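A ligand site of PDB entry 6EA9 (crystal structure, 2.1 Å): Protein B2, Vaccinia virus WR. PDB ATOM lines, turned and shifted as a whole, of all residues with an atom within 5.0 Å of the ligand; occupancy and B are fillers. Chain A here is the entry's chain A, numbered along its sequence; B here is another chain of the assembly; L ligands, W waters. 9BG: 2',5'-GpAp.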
ATOM      1  N   ASN A 129      -5.300  22.420 -15.226  1.00  0.00           N
ATOM      2  CA  ASN A 129      -5.275  23.868 -15.130  1.00  0.00           C
ATOM      3  C   ASN A 129      -6.548  24.455 -15.693  1.00  0.00           C
ATOM      4  O   ASN A 129      -7.136  23.947 -16.651  1.00  0.00           O
ATOM      5  CB  ASN A 129      -4.076  24.431 -15.878  1.00  0.00           C
ATOM      6  CG  ASN A 129      -2.859  24.570 -14.995  1.00  0.00           C
ATOM      7  OD1 ASN A 129      -2.889  24.215 -13.814  1.00  0.00           O
ATOM      8  ND2 ASN A 129      -1.761  25.043 -15.580  1.00  0.00           N
ATOM      9  N   ALA A 130      -6.953  25.582 -15.118  1.00  0.00           N
ATOM     10  CA  ALA A 130      -8.014  26.427 -15.635  1.00  0.00           C
ATOM     11  C   ALA A 130      -7.367  27.605 -16.345  1.00  0.00           C
ATOM     12  O   ALA A 130      -6.175  27.886 -16.170  1.00  0.00           O
ATOM     13  CB  ALA A 130      -8.938  26.905 -14.499  1.00  0.00           C
ATOM     14  N   VAL A 131      -8.158  28.297 -17.155  1.00  0.00           N
ATOM     15  CA  VAL A 131      -7.653  29.373 -17.995  1.00  0.00           C
ATOM     16  C   VAL A 131      -8.425  30.650 -17.683  1.00  0.00           C
ATOM     17  O   VAL A 131      -9.656  30.639 -17.653  1.00  0.00           O
ATOM     18  CB  VAL A 131      -7.776  29.039 -19.494  1.00  0.00           C
ATOM     19  CG1 VAL A 131      -7.457  30.268 -20.359  1.00  0.00           C
ATOM     20  CG2 VAL A 131      -6.888  27.870 -19.843  1.00  0.00           C
ATOM     21  N   TYR A 132      -7.693  31.745 -17.492  1.00  0.00           N
ATOM     22  CA  TYR A 132      -8.290  33.070 -17.555  1.00  0.00           C
ATOM     23  C   TYR A 132      -7.392  33.964 -18.401  1.00  0.00           C
ATOM     24  O   TYR A 132      -6.225  34.164 -18.054  1.00  0.00           O
ATOM     25  CB  TYR A 132      -8.478  33.692 -16.169  1.00  0.00           C
ATOM     26  CG  TYR A 132      -9.121  35.065 -16.253  1.00  0.00           C
ATOM     27  CD1 TYR A 132     -10.517  35.211 -16.273  1.00  0.00           C
ATOM     28  CD2 TYR A 132      -8.342  36.204 -16.369  1.00  0.00           C
ATOM     29  CE1 TYR A 132     -11.103  36.466 -16.391  1.00  0.00           C
ATOM     30  CE2 TYR A 132      -8.918  37.454 -16.479  1.00  0.00           C
ATOM     31  CZ  TYR A 132     -10.295  37.574 -16.490  1.00  0.00           C
ATOM     32  OH  TYR A 132     -10.844  38.825 -16.608  1.00  0.00           O
ATOM     33  N   TYR A 139      -7.567  25.911 -10.364  1.00  0.00           N
ATOM     34  CA  TYR A 139      -8.886  26.529 -10.324  1.00  0.00           C
ATOM     35  C   TYR A 139      -8.978  27.696  -9.351  1.00  0.00           C
ATOM     36  O   TYR A 139      -9.463  28.776  -9.714  1.00  0.00           O
ATOM     37  CB  TYR A 139      -9.935  25.469 -10.000  1.00  0.00           C
ATOM     38  CG  TYR A 139     -11.331  26.039  -9.956  1.00  0.00           C
ATOM     39  CD1 TYR A 139     -12.003  26.298 -11.134  1.00  0.00           C
ATOM     40  CD2 TYR A 139     -11.975  26.292  -8.749  1.00  0.00           C
ATOM     41  CE1 TYR A 139     -13.264  26.814 -11.121  1.00  0.00           C
ATOM     42  CE2 TYR A 139     -13.257  26.794  -8.732  1.00  0.00           C
ATOM     43  CZ  TYR A 139     -13.888  27.056  -9.922  1.00  0.00           C
ATOM     44  OH  TYR A 139     -15.153  27.565  -9.946  1.00  0.00           O
ATOM     45  N   ILE A 142      -7.273  30.822 -10.537  1.00  0.00           N
ATOM     46  CA  ILE A 142      -7.959  31.416 -11.692  1.00  0.00           C
ATOM     47  C   ILE A 142      -9.244  32.076 -11.248  1.00  0.00           C
ATOM     48  O   ILE A 142      -9.572  33.193 -11.672  1.00  0.00           O
ATOM     49  CB  ILE A 142      -8.206  30.346 -12.768  1.00  0.00           C
ATOM     50  CG1 ILE A 142      -6.883  29.903 -13.386  1.00  0.00           C
ATOM     51  CG2 ILE A 142      -9.171  30.871 -13.830  1.00  0.00           C
ATOM     52  CD1 ILE A 142      -6.090  31.039 -14.012  1.00  0.00           C
ATOM     53  N   LYS A 143      -9.988  31.405 -10.355  1.00  0.00           N
ATOM     54  CA  LYS A 143     -11.238  31.983  -9.861  1.00  0.00           C
ATOM     55  C   LYS A 143     -10.997  33.316  -9.177  1.00  0.00           C
ATOM     56  O   LYS A 143     -11.728  34.278  -9.422  1.00  0.00           O
ATOM     57  CB  LYS A 143     -11.925  31.011  -8.914  1.00  0.00           C
ATOM     58  CG  LYS A 143     -13.089  30.296  -9.539  1.00  0.00           C
ATOM     59  CD  LYS A 143     -14.182  31.311  -9.850  1.00  0.00           C
ATOM     60  CE  LYS A 143     -15.455  30.632 -10.236  1.00  0.00           C
ATOM     61  NZ  LYS A 143     -16.459  31.615 -10.652  1.00  0.00           N
ATOM     62  N   ALA A 146     -10.165  35.982 -11.830  1.00  0.00           N
ATOM     63  CA  ALA A 146     -11.351  36.418 -12.558  1.00  0.00           C
ATOM     64  C   ALA A 146     -12.178  37.393 -11.744  1.00  0.00           C
ATOM     65  O   ALA A 146     -12.686  38.387 -12.278  1.00  0.00           O
ATOM     66  CB  ALA A 146     -12.195  35.212 -12.957  1.00  0.00           C
ATOM     67  N   LYS A 147     -12.349  37.121 -10.447  1.00  0.00           N
ATOM     68  CA  LYS A 147     -13.143  38.023  -9.611  1.00  0.00           C
ATOM     69  C   LYS A 147     -12.459  39.374  -9.478  1.00  0.00           C
ATOM     70  O   LYS A 147     -13.123  40.423  -9.475  1.00  0.00           O
ATOM     71  CB  LYS A 147     -13.402  37.398  -8.236  1.00  0.00           C
ATOM     72  CG  LYS A 147     -14.225  36.096  -8.277  1.00  0.00           C
ATOM     73  CD  LYS A 147     -14.625  35.626  -6.873  1.00  0.00           C
ATOM     74  CE  LYS A 147     -13.686  34.599  -6.261  1.00  0.00           C
ATOM     75  NZ  LYS A 147     -12.405  35.211  -5.760  1.00  0.00           N
ATOM     76  N   ASN A 150     -13.053  41.521 -12.423  1.00  0.00           N
ATOM     77  CA  ASN A 150     -14.455  41.885 -12.596  1.00  0.00           C
ATOM     78  C   ASN A 150     -14.671  43.365 -12.331  1.00  0.00           C
ATOM     79  O   ASN A 150     -15.635  43.959 -12.847  1.00  0.00           O
ATOM     80  CB  ASN A 150     -15.327  41.033 -11.673  1.00  0.00           C
ATOM     81  CG  ASN A 150     -16.709  40.825 -12.230  1.00  0.00           C
ATOM     82  OD1 ASN A 150     -16.872  40.252 -13.313  1.00  0.00           O
ATOM     83  ND2 ASN A 150     -17.725  41.299 -11.512  1.00  0.00           N
ATOM     84  N   ILE A 168      -9.118  19.335 -23.586  1.00  0.00           N
ATOM     85  CA  ILE A 168      -9.919  20.484 -23.979  1.00  0.00           C
ATOM     86  C   ILE A 168      -9.007  21.484 -24.655  1.00  0.00           C
ATOM     87  O   ILE A 168      -7.815  21.567 -24.351  1.00  0.00           O
ATOM     88  CB  ILE A 168     -10.627  21.090 -22.737  1.00  0.00           C
ATOM     89  CG1 ILE A 168     -11.704  22.095 -23.146  1.00  0.00           C
ATOM     90  CG2 ILE A 168      -9.612  21.742 -21.778  1.00  0.00           C
ATOM     91  CD1 ILE A 168     -12.574  22.626 -21.921  1.00  0.00           C
ATOM     92  N   GLN A 170      -9.031  25.795 -25.692  1.00  0.00           N
ATOM     93  CA  GLN A 170      -9.712  27.054 -25.476  1.00  0.00           C
ATOM     94  C   GLN A 170      -9.029  28.174 -26.230  1.00  0.00           C
ATOM     95  O   GLN A 170      -7.823  28.131 -26.479  1.00  0.00           O
ATOM     96  CB  GLN A 170      -9.779  27.424 -23.988  1.00  0.00           C
ATOM     97  CG  GLN A 170     -10.429  26.384 -23.080  1.00  0.00           C
ATOM     98  CD  GLN A 170     -10.659  26.949 -21.702  1.00  0.00           C
ATOM     99  OE1 GLN A 170     -11.386  27.920 -21.577  1.00  0.00           O
ATOM    100  NE2 GLN A 170     -10.047  26.360 -20.671  1.00  0.00           N
ATOM    101  N   GLU A 180     -10.102  39.230 -19.477  1.00  0.00           N
ATOM    102  CA  GLU A 180     -10.626  38.329 -20.481  1.00  0.00           C
ATOM    103  C   GLU A 180     -11.868  38.924 -21.114  1.00  0.00           C
ATOM    104  O   GLU A 180     -12.894  39.115 -20.441  1.00  0.00           O
ATOM    105  CB  GLU A 180     -10.927  36.976 -19.859  1.00  0.00           C
ATOM    106  CG  GLU A 180     -11.555  35.979 -20.785  1.00  0.00           C
ATOM    107  CD  GLU A 180     -11.622  34.625 -20.125  1.00  0.00           C
ATOM    108  OE1 GLU A 180     -10.557  34.055 -19.861  1.00  0.00           O
ATOM    109  OE2 GLU A 180     -12.754  34.190 -19.798  1.00  0.00           O
ATOM    110  N   ARG A 183     -14.003  34.118 -24.353  1.00  0.00           N
ATOM    111  CA  ARG A 183     -13.504  32.759 -24.156  1.00  0.00           C
ATOM    112  C   ARG A 183     -14.362  31.826 -24.992  1.00  0.00           C
ATOM    113  O   ARG A 183     -15.581  31.779 -24.806  1.00  0.00           O
ATOM    114  CB  ARG A 183     -13.575  32.323 -22.701  1.00  0.00           C
ATOM    115  CG  ARG A 183     -13.144  30.871 -22.528  1.00  0.00           C
ATOM    116  CD  ARG A 183     -13.621  30.264 -21.188  1.00  0.00           C
ATOM    117  NE  ARG A 183     -13.277  31.133 -20.079  1.00  0.00           N
ATOM    118  CZ  ARG A 183     -12.294  30.900 -19.217  1.00  0.00           C
ATOM    119  NH1 ARG A 183     -12.060  31.753 -18.236  1.00  0.00           N
ATOM    120  NH2 ARG A 183     -11.518  29.823 -19.373  1.00  0.00           N
ATOM    121  N   ARG A 185     -14.527  27.587 -25.897  1.00  0.00           N
ATOM    122  CA  ARG A 185     -14.000  26.302 -25.485  1.00  0.00           C
ATOM    123  C   ARG A 185     -14.315  25.252 -26.538  1.00  0.00           C
ATOM    124  O   ARG A 185     -15.461  25.151 -26.992  1.00  0.00           O
ATOM    125  CB  ARG A 185     -14.581  25.870 -24.136  1.00  0.00           C
ATOM    126  CG  ARG A 185     -14.323  26.792 -22.927  1.00  0.00           C
ATOM    127  CD  ARG A 185     -14.853  26.116 -21.685  1.00  0.00           C
ATOM    128  NE  ARG A 185     -14.827  26.905 -20.443  1.00  0.00           N
ATOM    129  CZ  ARG A 185     -15.845  27.617 -19.981  1.00  0.00           C
ATOM    130  NH1 ARG A 185     -16.982  27.686 -20.675  1.00  0.00           N
ATOM    131  NH2 ARG A 185     -15.753  28.267 -18.822  1.00  0.00           N
ATOM    132  N   LYS A 187     -14.365  21.213 -26.955  1.00  0.00           N
ATOM    133  CA  LYS A 187     -14.355  20.052 -26.064  1.00  0.00           C
ATOM    134  C   LYS A 187     -13.710  18.846 -26.742  1.00  0.00           C
ATOM    135  O   LYS A 187     -14.325  17.809 -27.001  1.00  0.00           O
ATOM    136  CB  LYS A 187     -15.763  19.755 -25.566  1.00  0.00           C
ATOM    137  CG  LYS A 187     -16.442  20.947 -24.880  1.00  0.00           C
ATOM    138  CD  LYS A 187     -15.507  21.648 -23.902  1.00  0.00           C
ATOM    139  CE  LYS A 187     -16.247  22.643 -23.013  1.00  0.00           C
ATOM    140  NZ  LYS A 187     -17.031  21.897 -22.021  1.00  0.00           N
ATOM    141  N   TYR B  13     -27.493  34.042 -10.070  1.00  0.00           N
ATOM    142  CA  TYR B  13     -26.084  34.084 -10.465  1.00  0.00           C
ATOM    143  C   TYR B  13     -25.190  34.474  -9.295  1.00  0.00           C
ATOM    144  O   TYR B  13     -25.463  35.446  -8.581  1.00  0.00           O
ATOM    145  CB  TYR B  13     -25.867  35.060 -11.629  1.00  0.00           C
ATOM    146  CG  TYR B  13     -24.390  35.259 -11.912  1.00  0.00           C
ATOM    147  CD1 TYR B  13     -23.625  34.247 -12.470  1.00  0.00           C
ATOM    148  CD2 TYR B  13     -23.761  36.449 -11.573  1.00  0.00           C
ATOM    149  CE1 TYR B  13     -22.275  34.417 -12.713  1.00  0.00           C
ATOM    150  CE2 TYR B  13     -22.404  36.632 -11.816  1.00  0.00           C
ATOM    151  CZ  TYR B  13     -21.670  35.612 -12.378  1.00  0.00           C
ATOM    152  OH  TYR B  13     -20.327  35.793 -12.617  1.00  0.00           O
ATOM    153  N   GLU B  15     -20.906  34.827  -8.705  1.00  0.00           N
ATOM    154  CA  GLU B  15     -19.582  34.759  -9.340  1.00  0.00           C
ATOM    155  C   GLU B  15     -18.680  33.712  -8.708  1.00  0.00           C
ATOM    156  O   GLU B  15     -17.743  33.240  -9.365  1.00  0.00           O
ATOM    157  CB  GLU B  15     -18.892  36.131  -9.261  1.00  0.00           C
ATOM    158  CG  GLU B  15     -18.555  36.512  -7.826  1.00  0.00           C
ATOM    159  CD  GLU B  15     -17.839  37.838  -7.713  1.00  0.00           C
ATOM    160  OE1 GLU B  15     -17.513  38.238  -6.564  1.00  0.00           O
ATOM    161  OE2 GLU B  15     -17.614  38.484  -8.745  1.00  0.00           O
ATOM    162  N   LEU B  17     -19.530  30.679  -7.833  1.00  0.00           N
ATOM    163  CA  LEU B  17     -19.947  29.321  -8.164  1.00  0.00           C
ATOM    164  C   LEU B  17     -19.594  29.026  -9.618  1.00  0.00           C
ATOM    165  O   LEU B  17     -19.226  29.904 -10.391  1.00  0.00           O
ATOM    166  CB  LEU B  17     -21.459  29.164  -7.943  1.00  0.00           C
ATOM    167  CG  LEU B  17     -22.030  29.389  -6.543  1.00  0.00           C
ATOM    168  CD1 LEU B  17     -23.515  29.017  -6.502  1.00  0.00           C
ATOM    169  CD2 LEU B  17     -21.241  28.653  -5.471  1.00  0.00           C
ATOM    170  N   HIS B  18     -19.665  27.743  -9.987  1.00  0.00           N
ATOM    171  CA  HIS B  18     -19.501  27.349 -11.380  1.00  0.00           C
ATOM    172  C   HIS B  18     -20.624  27.967 -12.204  1.00  0.00           C
ATOM    173  O   HIS B  18     -21.775  28.046 -11.759  1.00  0.00           O
ATOM    174  CB  HIS B  18     -19.498  25.830 -11.496  1.00  0.00           C
ATOM    175  CG  HIS B  18     -18.487  25.175 -10.607  1.00  0.00           C
ATOM    176  ND1 HIS B  18     -17.131  25.206 -10.860  1.00  0.00           N
ATOM    177  CD2 HIS B  18     -18.643  24.479  -9.450  1.00  0.00           C
ATOM    178  CE1 HIS B  18     -16.496  24.558  -9.893  1.00  0.00           C
ATOM    179  NE2 HIS B  18     -17.394  24.102  -9.024  1.00  0.00           N
ATOM    180  N   ALA B  19     -20.291  28.427 -13.412  1.00  0.00           N
ATOM    181  CA  ALA B  19     -21.252  29.127 -14.273  1.00  0.00           C
ATOM    182  C   ALA B  19     -21.499  28.350 -15.562  1.00  0.00           C
ATOM    183  O   ALA B  19     -20.571  28.105 -16.330  1.00  0.00           O
ATOM    184  CB  ALA B  19     -20.751  30.538 -14.600  1.00  0.00           C
ATOM    185  N   PHE B  20     -22.754  28.022 -15.810  1.00  0.00           N
ATOM    186  CA  PHE B  20     -23.222  27.384 -17.042  1.00  0.00           C
ATOM    187  C   PHE B  20     -24.428  28.177 -17.510  1.00  0.00           C
ATOM    188  O   PHE B  20     -24.935  29.039 -16.785  1.00  0.00           O
ATOM    189  CB  PHE B  20     -23.585  25.925 -16.782  1.00  0.00           C
ATOM    190  CG  PHE B  20     -22.596  25.202 -15.909  1.00  0.00           C
ATOM    191  CD1 PHE B  20     -21.337  24.866 -16.394  1.00  0.00           C
ATOM    192  CD2 PHE B  20     -22.931  24.840 -14.612  1.00  0.00           C
ATOM    193  CE1 PHE B  20     -20.423  24.197 -15.587  1.00  0.00           C
ATOM    194  CE2 PHE B  20     -22.031  24.170 -13.802  1.00  0.00           C
ATOM    195  CZ  PHE B  20     -20.775  23.852 -14.295  1.00  0.00           C
ATOM    196  N   ALA B  28     -19.745  20.934 -10.604  1.00  0.00           N
ATOM    197  CA  ALA B  28     -19.545  21.030 -12.044  1.00  0.00           C
ATOM    198  C   ALA B  28     -19.768  19.649 -12.650  1.00  0.00           C
ATOM    199  O   ALA B  28     -18.851  18.834 -12.695  1.00  0.00           O
ATOM    200  CB  ALA B  28     -18.155  21.562 -12.350  1.00  0.00           C
ATOM    201  N   ARG B  61     -22.135  39.706 -18.169  1.00  0.00           N
ATOM    202  CA  ARG B  61     -21.379  38.533 -18.589  1.00  0.00           C
ATOM    203  C   ARG B  61     -22.289  37.611 -19.400  1.00  0.00           C
ATOM    204  O   ARG B  61     -23.405  37.297 -18.969  1.00  0.00           O
ATOM    205  CB  ARG B  61     -20.817  37.829 -17.352  1.00  0.00           C
ATOM    206  CG  ARG B  61     -20.263  36.475 -17.592  1.00  0.00           C
ATOM    207  CD  ARG B  61     -19.722  35.831 -16.315  1.00  0.00           C
ATOM    208  NE  ARG B  61     -19.015  34.604 -16.662  1.00  0.00           N
ATOM    209  CZ  ARG B  61     -18.608  33.690 -15.799  1.00  0.00           C
ATOM    210  NH1 ARG B  61     -18.844  33.843 -14.505  1.00  0.00           N
ATOM    211  NH2 ARG B  61     -17.965  32.600 -16.234  1.00  0.00           N
ATOM    212  N   ILE B 106     -21.478  21.315 -17.498  1.00  0.00           N
ATOM    213  CA  ILE B 106     -20.347  21.305 -18.426  1.00  0.00           C
ATOM    214  C   ILE B 106     -20.776  20.543 -19.676  1.00  0.00           C
ATOM    215  O   ILE B 106     -20.963  19.325 -19.623  1.00  0.00           O
ATOM    216  CB  ILE B 106     -19.085  20.699 -17.801  1.00  0.00           C
ATOM    217  CG1 ILE B 106     -18.568  21.613 -16.695  1.00  0.00           C
ATOM    218  CG2 ILE B 106     -17.967  20.472 -18.873  1.00  0.00           C
ATOM    219  CD1 ILE B 106     -17.324  21.075 -15.993  1.00  0.00           C
ATOM    220  N   GLY B 107     -20.967  21.262 -20.779  1.00  0.00           N
ATOM    221  CA  GLY B 107     -21.500  20.651 -21.975  1.00  0.00           C
ATOM    222  C   GLY B 107     -20.497  20.650 -23.113  1.00  0.00           C
ATOM    223  O   GLY B 107     -19.305  20.396 -22.902  1.00  0.00           O
ATOM    224  N   TYR B 108     -20.953  21.011 -24.311  1.00  0.00           N
ATOM    225  CA  TYR B 108     -20.067  20.983 -25.478  1.00  0.00           C
ATOM    226  C   TYR B 108     -19.520  22.386 -25.723  1.00  0.00           C
ATOM    227  O   TYR B 108     -19.288  23.136 -24.768  1.00  0.00           O
ATOM    228  CB  TYR B 108     -20.821  20.423 -26.685  1.00  0.00           C
ATOM    229  CG  TYR B 108     -21.262  18.989 -26.435  1.00  0.00           C
ATOM    230  CD1 TYR B 108     -20.387  17.940 -26.599  1.00  0.00           C
ATOM    231  CD2 TYR B 108     -22.561  18.699 -25.994  1.00  0.00           C
ATOM    232  CE1 TYR B 108     -20.767  16.633 -26.366  1.00  0.00           C
ATOM    233  CE2 TYR B 108     -22.958  17.385 -25.745  1.00  0.00           C
ATOM    234  CZ  TYR B 108     -22.051  16.359 -25.921  1.00  0.00           C
ATOM    235  OH  TYR B 108     -22.403  15.045 -25.692  1.00  0.00           O
ATOM    236  N   SER B 110     -18.529  26.141 -26.137  1.00  0.00           N
ATOM    237  CA  SER B 110     -19.114  27.228 -25.355  1.00  0.00           C
ATOM    238  C   SER B 110     -18.535  28.573 -25.782  1.00  0.00           C
ATOM    239  O   SER B 110     -17.467  28.663 -26.427  1.00  0.00           O
ATOM    240  CB  SER B 110     -18.890  27.047 -23.848  1.00  0.00           C
ATOM    241  OG  SER B 110     -17.537  27.253 -23.495  1.00  0.00           O
ATOM    242  N   ASP B 112     -18.164  32.538 -23.932  1.00  0.00           N
ATOM    243  CA  ASP B 112     -18.305  33.477 -22.824  1.00  0.00           C
ATOM    244  C   ASP B 112     -17.805  34.831 -23.293  1.00  0.00           C
ATOM    245  O   ASP B 112     -16.811  34.926 -24.012  1.00  0.00           O
ATOM    246  CB  ASP B 112     -17.502  32.998 -21.597  1.00  0.00           C
ATOM    247  CG  ASP B 112     -18.182  31.845 -20.867  1.00  0.00           C
ATOM    248  OD1 ASP B 112     -18.323  30.756 -21.460  1.00  0.00           O
ATOM    249  OD2 ASP B 112     -18.545  32.023 -19.677  1.00  0.00           O
HETATM  250  C10 9BG L   1     -14.421  22.866 -18.622  1.00  0.00           C
HETATM  251  C17 9BG L   1     -12.706  24.676 -14.591  1.00  0.00           C
HETATM  252  C24 9BG L   1     -13.175  29.394 -14.818  1.00  0.00           C
HETATM  253  C02 9BG L   1     -17.490  24.574 -19.379  1.00  0.00           C
HETATM  254  C04 9BG L   1     -17.505  25.998 -17.331  1.00  0.00           C
HETATM  255  C07 9BG L   1     -15.606  24.356 -17.733  1.00  0.00           C
HETATM  256  C08 9BG L   1     -16.200  23.952 -18.941  1.00  0.00           C
HETATM  257  C12 9BG L   1     -13.542  23.697 -16.499  1.00  0.00           C
HETATM  258  C14 9BG L   1     -13.304  23.597 -14.095  1.00  0.00           C
HETATM  259  C19 9BG L   1     -13.178  24.867 -16.113  1.00  0.00           C
HETATM  260  C23 9BG L   1     -12.374  29.178 -16.109  1.00  0.00           C
HETATM  261  C25 9BG L   1     -14.418  29.092 -14.992  1.00  0.00           C
HETATM  262  N34 9BG L   1     -14.735  32.753 -14.928  1.00  0.00           N
HETATM  263  O01 9BG L   1     -18.020  24.250 -20.376  1.00  0.00           O
HETATM  264  N03 9BG L   1     -18.117  25.596 -18.551  1.00  0.00           N
HETATM  265  N05 9BG L   1     -18.111  27.009 -16.510  1.00  0.00           N
HETATM  266  N06 9BG L   1     -16.267  25.388 -16.893  1.00  0.00           N
HETATM  267  N09 9BG L   1     -15.445  23.049 -19.455  1.00  0.00           N
HETATM  268  N11 9BG L   1     -14.513  23.659 -17.606  1.00  0.00           N
HETATM  269  O13 9BG L   1     -14.149  23.038 -15.213  1.00  0.00           O
HETATM  270  C15 9BG L   1     -14.207  23.977 -12.912  1.00  0.00           C
HETATM  271  O16 9BG L   1     -15.293  23.108 -12.901  1.00  0.00           O
HETATM  272  O18 9BG L   1     -11.203  24.433 -14.606  1.00  0.00           O
HETATM  273  O20 9BG L   1     -11.961  25.277 -16.884  1.00  0.00           O
HETATM  274  P21 9BG L   1     -11.887  26.877 -17.340  1.00  0.00           P
HETATM  275  O22 9BG L   1     -11.968  27.827 -15.950  1.00  0.00           O
HETATM  276  O26 9BG L   1     -14.864  28.693 -13.680  1.00  0.00           O
HETATM  277  P27 9BG L   1     -16.425  28.164 -13.249  1.00  0.00           P
HETATM  278  O28 9BG L   1     -17.520  28.896 -14.034  1.00  0.00           O
HETATM  279  O29 9BG L   1     -16.572  28.520 -11.684  1.00  0.00           O
HETATM  280  O30 9BG L   1     -16.566  26.753 -13.385  1.00  0.00           O
HETATM  281  C31 9BG L   1     -15.043  30.523 -15.457  1.00  0.00           C
HETATM  282  O32 9BG L   1     -16.453  30.518 -15.457  1.00  0.00           O
HETATM  283  C33 9BG L   1     -14.547  31.342 -14.541  1.00  0.00           C
HETATM  284  C35 9BG L   1     -15.261  33.659 -14.081  1.00  0.00           C
HETATM  285  N36 9BG L   1     -15.659  33.536 -12.821  1.00  0.00           N
HETATM  286  C37 9BG L   1     -16.150  34.589 -12.151  1.00  0.00           C
HETATM  287  N38 9BG L   1     -16.237  35.762 -12.750  1.00  0.00           N
HETATM  288  C39 9BG L   1     -15.866  35.970 -14.007  1.00  0.00           C
HETATM  289  N40 9BG L   1     -16.003  37.320 -14.612  1.00  0.00           N
HETATM  290  C41 9BG L   1     -15.335  34.879 -14.749  1.00  0.00           C
HETATM  291  N42 9BG L   1     -14.856  34.657 -15.987  1.00  0.00           N
HETATM  292  C43 9BG L   1     -14.495  33.350 -16.070  1.00  0.00           C
HETATM  293  O44 9BG L   1     -13.110  30.928 -14.440  1.00  0.00           O
HETATM  294  O45 9BG L   1     -10.584  27.226 -18.035  1.00  0.00           O
HETATM  295  O46 9BG L   1     -13.132  27.207 -18.194  1.00  0.00           O
HETATM  296  O   HOH W   1     -20.401  26.749 -19.317  1.00  0.00           O
HETATM  297  O   HOH W   2     -20.107  23.569 -21.977  1.00  0.00           O
HETATM  298  O   HOH W   3     -18.368  29.779 -18.600  1.00  0.00           O
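O of Leu 17 of chain B sits close to O29 of the ligand, 3.3 Å away. Merely in contact with the ligand: Ala 130, Ile 142, Ala 146, Ile 168, Glu 15 of chain B, Phe 20 of chain B, Ala 28 of chain B and Ile 106 of chain B. Hydrophobic or aromatic side chains within 4 Å of the ligand: Ala 130, Val 131, Tyr 139, Ile 142, Ala 146, Ile 168, His 18 of chain B, Ala 19 of chain B, Phe 20 of chain B, Ala 28 of chain B and Ile 106 of chain B. Within 4 Å of the ligand: Ala 130, Val 131, Tyr 139, Ile 142, Lys 143, Ala 146, Asn 150, Ile 168, Gln 170, Arg 183, Arg 185, Lys 187, Glu 15 of chain B, Leu 17 of chain B, His 18 of chain B, Ala 19 of chain B, Phe 20 of chain B, Ala 28 of chain B, Arg 61 of chain B and Ile 106 of chain B.
A ring nitrogen (ND1) of His 18 of chain B is in hydrogen-bond range of the side-chain hydroxyl of Tyr 139 (3.2 Å). OD2 of Asp 112 of chain B is in salt-bridge range of NH2 of Arg 61 of chain B (3.5 Å). NZ of Lys 143 is in hydrogen-bond range of O of Leu 17 of chain B. The side-chain amino group (NZ) of Lys 143 lies within hydrogen-bond range of the backbone carbonyl oxygen (O) of Glu 15 of chain B (2.4 Å). NH2 of Arg 183 is in hydrogen-bond range of O of Val 131, 2.7 Å away. NH2 of Arg 183 is in hydrogen-bond range of OE1 of Gln 170. OG of Ser 110 of chain B is in hydrogen-bond range of NH1 of Arg 185, at 2.9 Å. N of Asp 112 of chain B lies within hydrogen-bond range of O of Arg 183 (2.8 Å).
The side-chain hydroxyl of Tyr 139 lies within hydrogen-bond range of an oxygen (O29) of the ligand. The guanidinium group (NH2) of Arg 61 of chain B lies within hydrogen-bond range of an oxygen (O32) of the ligand (2.7 Å). N of Ala 19 of chain B sits at hydrogen-bond distance from O28 of the ligand (2.9 Å). N05 of the ligand lies within hydrogen-bond range of O of Ala 19 of chain B, 2.7 Å away. An oxygen (O29) of the ligand lies within salt-bridge range of the side-chain amino group (NZ) of Lys 143. An oxygen (O45) of the ligand sits at hydrogen-bond distance from the backbone NH of Val 131 (2.8 Å). NE2 of Gln 170 is in hydrogen-bond range of O45 of the ligand. An oxygen (O46) of the ligand is in salt-bridge range of the guanidinium group of Arg 185 (2.8 Å). A ring nitrogen (ND1) of His 18 of chain B sits at hydrogen-bond distance from an oxygen (O30) of the ligand (3.0 Å). NZ of Lys 187 is in hydrogen-bond range of O01 of the ligand. An oxygen (O45) of the ligand lies within salt-bridge range of the guanidinium group (NH2) of Arg 183 (3.1 Å). OD1 of Asn 150 sits at hydrogen-bond distance from N40 of the ligand (3.3 Å).
Water W1 bridges a nitrogen (N03) of the ligand (2.7 Å) and the backbone carbonyl oxygen of Ala 19 of chain B (3.3 Å). Water W2 lies within hydrogen-bond range of O01 of the ligand, N of Gly 107 of chain B and O of Tyr 108 of chain B. Water W3 lies within hydrogen-bond range of OD2 of Asp 112 of chain B (2.5 Å), NH2 of Arg 185 (3.0 Å) and N05 of the ligand (3.5 Å).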
